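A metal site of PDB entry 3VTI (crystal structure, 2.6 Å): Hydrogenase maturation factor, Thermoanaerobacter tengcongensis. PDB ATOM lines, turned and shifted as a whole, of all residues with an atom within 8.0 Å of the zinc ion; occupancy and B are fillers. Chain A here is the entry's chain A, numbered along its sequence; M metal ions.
Within 4 Å of the zinc ion: Cys 164, Cys 167, Cys 186 and Cys 189.
Along chain A the residues within 4 Å of the zinc ion span positions 164 to 189.
The nearest printed residue that does not touch the zinc ion is Arg 127 (4.2 Å).
The side-chain sulfur (SG) of Cys 164 sits close to the backbone NH (N) of Lys 166 (3.8 Å).
SG of Cys 186 lies close to NH1 of Arg 127 (3.3 Å).
The side-chain sulfur (SG) of Cys 167 lies close to the guanidinium group (NH2) of Arg 128.
The backbone carbonyl oxygen (O) of Cys 186 sits at hydrogen-bond distance from the side-chain hydroxyl (OH) of Tyr 131 (3.1 Å).
The side-chain sulfur (SG) of Cys 186 sits close to the backbone NH (N) of Asp 188.
The zinc ion is bound by the side-chain sulfur of Cys 189, the side-chain sulfur of Cys 167, the side-chain sulfur of Cys 164 and the side-chain sulfur of Cys 186.
The zinc ion has four donor atoms within binding distance.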
ATOM      1  N   ARG A 127     -23.186   1.343  11.540  1.00  0.00           N
ATOM      2  CA  ARG A 127     -22.055   0.470  11.196  1.00  0.00           C
ATOM      3  C   ARG A 127     -22.408  -0.716  10.261  1.00  0.00           C
ATOM      4  O   ARG A 127     -21.555  -1.209   9.518  1.00  0.00           O
ATOM      5  CB  ARG A 127     -21.424  -0.027  12.500  1.00  0.00           C
ATOM      6  CG  ARG A 127     -20.208  -0.921  12.337  1.00  0.00           C
ATOM      7  CD  ARG A 127     -19.620  -1.292  13.683  1.00  0.00           C
ATOM      8  NE  ARG A 127     -20.486  -2.180  14.461  1.00  0.00           N
ATOM      9  CZ  ARG A 127     -20.300  -3.494  14.567  1.00  0.00           C
ATOM     10  NH1 ARG A 127     -19.293  -4.081  13.934  1.00  0.00           N
ATOM     11  NH2 ARG A 127     -21.123  -4.225  15.316  1.00  0.00           N
ATOM     12  N   ARG A 128     -23.667  -1.161  10.297  1.00  0.00           N
ATOM     13  CA  ARG A 128     -24.124  -2.284   9.455  1.00  0.00           C
ATOM     14  C   ARG A 128     -24.931  -1.846   8.228  1.00  0.00           C
ATOM     15  O   ARG A 128     -25.643  -2.657   7.628  1.00  0.00           O
ATOM     16  CB  ARG A 128     -24.921  -3.295  10.273  1.00  0.00           C
ATOM     17  CG  ARG A 128     -24.088  -4.090  11.257  1.00  0.00           C
ATOM     18  CD  ARG A 128     -24.896  -5.191  11.875  1.00  0.00           C
ATOM     19  NE  ARG A 128     -24.104  -6.004  12.790  1.00  0.00           N
ATOM     20  CZ  ARG A 128     -23.885  -5.705  14.074  1.00  0.00           C
ATOM     21  NH1 ARG A 128     -24.373  -4.586  14.612  1.00  0.00           N
ATOM     22  NH2 ARG A 128     -23.159  -6.539  14.817  1.00  0.00           N
ATOM     23  N   TYR A 131     -25.251  -3.993   5.055  1.00  0.00           N
ATOM     24  CA  TYR A 131     -24.612  -5.276   5.337  1.00  0.00           C
ATOM     25  C   TYR A 131     -25.557  -6.458   5.052  1.00  0.00           C
ATOM     26  O   TYR A 131     -26.589  -6.592   5.694  1.00  0.00           O
ATOM     27  CB  TYR A 131     -24.041  -5.341   6.756  1.00  0.00           C
ATOM     28  CG  TYR A 131     -23.361  -6.664   7.030  1.00  0.00           C
ATOM     29  CD1 TYR A 131     -23.877  -7.557   7.963  1.00  0.00           C
ATOM     30  CD2 TYR A 131     -22.218  -7.034   6.308  1.00  0.00           C
ATOM     31  CE1 TYR A 131     -23.262  -8.782   8.199  1.00  0.00           C
ATOM     32  CE2 TYR A 131     -21.612  -8.258   6.521  1.00  0.00           C
ATOM     33  CZ  TYR A 131     -22.128  -9.112   7.469  1.00  0.00           C
ATOM     34  OH  TYR A 131     -21.503 -10.310   7.663  1.00  0.00           O
ATOM     35  N   ARG A 153     -23.525 -20.783  18.602  1.00  0.00           N
ATOM     36  CA  ARG A 153     -22.661 -20.471  17.458  1.00  0.00           C
ATOM     37  C   ARG A 153     -21.703 -21.612  17.078  1.00  0.00           C
ATOM     38  O   ARG A 153     -21.540 -21.928  15.885  1.00  0.00           O
ATOM     39  CB  ARG A 153     -21.858 -19.202  17.720  1.00  0.00           C
ATOM     40  CG  ARG A 153     -21.083 -18.689  16.519  1.00  0.00           C
ATOM     41  CD  ARG A 153     -20.413 -17.398  16.854  1.00  0.00           C
ATOM     42  NE  ARG A 153     -19.630 -16.872  15.747  1.00  0.00           N
ATOM     43  CZ  ARG A 153     -20.017 -15.866  14.965  1.00  0.00           C
ATOM     44  NH1 ARG A 153     -21.199 -15.273  15.136  1.00  0.00           N
ATOM     45  NH2 ARG A 153     -19.208 -15.440  13.997  1.00  0.00           N
ATOM     46  N   PRO A 162     -14.498 -16.027  13.471  1.00  0.00           N
ATOM     47  CA  PRO A 162     -14.318 -15.436  14.797  1.00  0.00           C
ATOM     48  C   PRO A 162     -14.925 -14.027  14.852  1.00  0.00           C
ATOM     49  O   PRO A 162     -14.713 -13.218  13.943  1.00  0.00           O
ATOM     50  CB  PRO A 162     -12.788 -15.371  14.952  1.00  0.00           C
ATOM     51  CG  PRO A 162     -12.253 -15.388  13.559  1.00  0.00           C
ATOM     52  CD  PRO A 162     -13.239 -16.196  12.739  1.00  0.00           C
ATOM     53  N   MET A 163     -15.706 -13.773  15.905  1.00  0.00           N
ATOM     54  CA  MET A 163     -16.287 -12.455  16.135  1.00  0.00           C
ATOM     55  C   MET A 163     -15.226 -11.373  16.303  1.00  0.00           C
ATOM     56  O   MET A 163     -14.162 -11.633  16.872  1.00  0.00           O
ATOM     57  CB  MET A 163     -17.153 -12.471  17.395  1.00  0.00           C
ATOM     58  CG  MET A 163     -18.499 -13.107  17.200  1.00  0.00           C
ATOM     59  SD  MET A 163     -19.479 -13.057  18.705  1.00  0.00           S
ATOM     60  CE  MET A 163     -18.719 -14.373  19.669  1.00  0.00           C
ATOM     61  N   CYS A 164     -15.521 -10.183  15.793  1.00  0.00           N
ATOM     62  CA  CYS A 164     -14.707  -8.997  16.035  1.00  0.00           C
ATOM     63  C   CYS A 164     -15.109  -8.443  17.400  1.00  0.00           C
ATOM     64  O   CYS A 164     -16.082  -8.916  17.995  1.00  0.00           O
ATOM     65  CB  CYS A 164     -14.916  -7.944  14.943  1.00  0.00           C
ATOM     66  SG  CYS A 164     -16.542  -7.157  14.930  1.00  0.00           S
ATOM     67  N   GLU A 165     -14.360  -7.442  17.874  1.00  0.00           N
ATOM     68  CA  GLU A 165     -14.579  -6.838  19.181  1.00  0.00           C
ATOM     69  C   GLU A 165     -15.972  -6.265  19.330  1.00  0.00           C
ATOM     70  O   GLU A 165     -16.670  -6.540  20.300  1.00  0.00           O
ATOM     71  CB  GLU A 165     -13.570  -5.701  19.404  1.00  0.00           C
ATOM     72  CG  GLU A 165     -12.133  -6.041  19.049  1.00  0.00           C
ATOM     73  CD  GLU A 165     -11.413  -6.808  20.133  1.00  0.00           C
ATOM     74  OE1 GLU A 165     -11.912  -7.896  20.526  1.00  0.00           O
ATOM     75  OE2 GLU A 165     -10.351  -6.313  20.604  1.00  0.00           O
ATOM     76  N   LYS A 166     -16.357  -5.465  18.327  1.00  0.00           N
ATOM     77  CA  LYS A 166     -17.599  -4.717  18.299  1.00  0.00           C
ATOM     78  C   LYS A 166     -18.813  -5.655  18.346  1.00  0.00           C
ATOM     79  O   LYS A 166     -19.800  -5.372  19.028  1.00  0.00           O
ATOM     80  CB  LYS A 166     -17.631  -3.863  17.029  1.00  0.00           C
ATOM     81  CG  LYS A 166     -18.276  -2.491  17.193  1.00  0.00           C
ATOM     82  CD  LYS A 166     -17.239  -1.374  17.240  1.00  0.00           C
ATOM     83  CE  LYS A 166     -16.650  -1.065  15.863  1.00  0.00           C
ATOM     84  NZ  LYS A 166     -15.844   0.192  15.893  1.00  0.00           N
ATOM     85  N   CYS A 167     -18.746  -6.772  17.618  1.00  0.00           N
ATOM     86  CA  CYS A 167     -19.819  -7.774  17.632  1.00  0.00           C
ATOM     87  C   CYS A 167     -19.815  -8.567  18.931  1.00  0.00           C
ATOM     88  O   CYS A 167     -20.862  -8.996  19.412  1.00  0.00           O
ATOM     89  CB  CYS A 167     -19.694  -8.742  16.449  1.00  0.00           C
ATOM     90  SG  CYS A 167     -20.089  -8.055  14.857  1.00  0.00           S
ATOM     91  N   SER A 168     -18.619  -8.759  19.505  1.00  0.00           N
ATOM     92  CA  SER A 168     -18.467  -9.567  20.705  1.00  0.00           C
ATOM     93  C   SER A 168     -19.145  -8.953  21.927  1.00  0.00           C
ATOM     94  O   SER A 168     -19.807  -9.655  22.703  1.00  0.00           O
ATOM     95  CB  SER A 168     -16.981  -9.834  20.984  1.00  0.00           C
ATOM     96  OG  SER A 168     -16.832 -10.717  22.078  1.00  0.00           O
ATOM     97  N   GLU A 170     -21.557  -6.703  21.916  1.00  0.00           N
ATOM     98  CA  GLU A 170     -23.002  -6.716  21.621  1.00  0.00           C
ATOM     99  C   GLU A 170     -23.619  -8.055  22.016  1.00  0.00           C
ATOM    100  O   GLU A 170     -24.671  -8.111  22.641  1.00  0.00           O
ATOM    101  CB  GLU A 170     -23.248  -6.461  20.125  1.00  0.00           C
ATOM    102  CG  GLU A 170     -23.086  -5.019  19.661  1.00  0.00           C
ATOM    103  CD  GLU A 170     -23.300  -4.880  18.157  1.00  0.00           C
ATOM    104  OE1 GLU A 170     -22.522  -5.471  17.374  1.00  0.00           O
ATOM    105  OE2 GLU A 170     -24.245  -4.163  17.754  1.00  0.00           O
ATOM    106  N   VAL A 184     -24.404 -13.388  14.696  1.00  0.00           N
ATOM    107  CA  VAL A 184     -23.992 -11.977  14.556  1.00  0.00           C
ATOM    108  C   VAL A 184     -22.804 -11.792  13.634  1.00  0.00           C
ATOM    109  O   VAL A 184     -21.880 -12.616  13.622  1.00  0.00           O
ATOM    110  CB  VAL A 184     -23.638 -11.269  15.902  1.00  0.00           C
ATOM    111  CG1 VAL A 184     -24.901 -10.742  16.556  1.00  0.00           C
ATOM    112  CG2 VAL A 184     -22.797 -12.167  16.836  1.00  0.00           C
ATOM    113  N   ALA A 185     -22.846 -10.685  12.896  1.00  0.00           N
ATOM    114  CA  ALA A 185     -21.850 -10.349  11.881  1.00  0.00           C
ATOM    115  C   ALA A 185     -21.890  -8.865  11.507  1.00  0.00           C
ATOM    116  O   ALA A 185     -22.873  -8.169  11.742  1.00  0.00           O
ATOM    117  CB  ALA A 185     -22.056 -11.215  10.639  1.00  0.00           C
ATOM    118  N   CYS A 186     -20.775  -8.395  10.946  1.00  0.00           N
ATOM    119  CA  CYS A 186     -20.659  -7.080  10.359  1.00  0.00           C
ATOM    120  C   CYS A 186     -19.725  -7.263   9.164  1.00  0.00           C
ATOM    121  O   CYS A 186     -19.318  -8.390   8.870  1.00  0.00           O
ATOM    122  CB  CYS A 186     -20.073  -6.091  11.366  1.00  0.00           C
ATOM    123  SG  CYS A 186     -18.345  -6.373  11.832  1.00  0.00           S
ATOM    124  N   PHE A 187     -19.393  -6.181   8.458  1.00  0.00           N
ATOM    125  CA  PHE A 187     -18.416  -6.253   7.368  1.00  0.00           C
ATOM    126  C   PHE A 187     -17.041  -6.780   7.820  1.00  0.00           C
ATOM    127  O   PHE A 187     -16.351  -7.462   7.063  1.00  0.00           O
ATOM    128  CB  PHE A 187     -18.249  -4.887   6.690  1.00  0.00           C
ATOM    129  CG  PHE A 187     -19.426  -4.459   5.842  1.00  0.00           C
ATOM    130  CD1 PHE A 187     -19.601  -4.978   4.555  1.00  0.00           C
ATOM    131  CD2 PHE A 187     -20.345  -3.535   6.317  1.00  0.00           C
ATOM    132  CE1 PHE A 187     -20.685  -4.575   3.768  1.00  0.00           C
ATOM    133  CE2 PHE A 187     -21.431  -3.135   5.539  1.00  0.00           C
ATOM    134  CZ  PHE A 187     -21.595  -3.652   4.266  1.00  0.00           C
ATOM    135  N   ASP A 188     -16.659  -6.467   9.061  1.00  0.00           N
ATOM    136  CA  ASP A 188     -15.312  -6.777   9.539  1.00  0.00           C
ATOM    137  C   ASP A 188     -15.080  -8.249   9.885  1.00  0.00           C
ATOM    138  O   ASP A 188     -13.957  -8.733   9.778  1.00  0.00           O
ATOM    139  CB  ASP A 188     -14.917  -5.877  10.728  1.00  0.00           C
ATOM    140  CG  ASP A 188     -15.104  -4.376  10.445  1.00  0.00           C
ATOM    141  OD1 ASP A 188     -15.399  -3.637  11.400  1.00  0.00           O
ATOM    142  OD2 ASP A 188     -14.941  -3.938   9.285  1.00  0.00           O
ATOM    143  N   CYS A 189     -16.131  -8.952  10.280  1.00  0.00           N
ATOM    144  CA  CYS A 189     -15.979 -10.343  10.741  1.00  0.00           C
ATOM    145  C   CYS A 189     -16.903 -11.347  10.084  1.00  0.00           C
ATOM    146  O   CYS A 189     -16.627 -12.545  10.077  1.00  0.00           O
ATOM    147  CB  CYS A 189     -16.135 -10.428  12.268  1.00  0.00           C
ATOM    148  SG  CYS A 189     -17.807 -10.166  12.879  1.00  0.00           S
ATOM    149  N   GLY A 190     -18.011 -10.857   9.521  1.00  0.00           N
ATOM    150  CA  GLY A 190     -19.019 -11.752   8.990  1.00  0.00           C
ATOM    151  C   GLY A 190     -18.823 -12.241   7.561  1.00  0.00           C
ATOM    152  O   GLY A 190     -17.811 -11.943   6.937  1.00  0.00           O
HETATM  153 ZN    ZN M   1     -18.213  -8.102  13.582  1.00  0.00          ZN
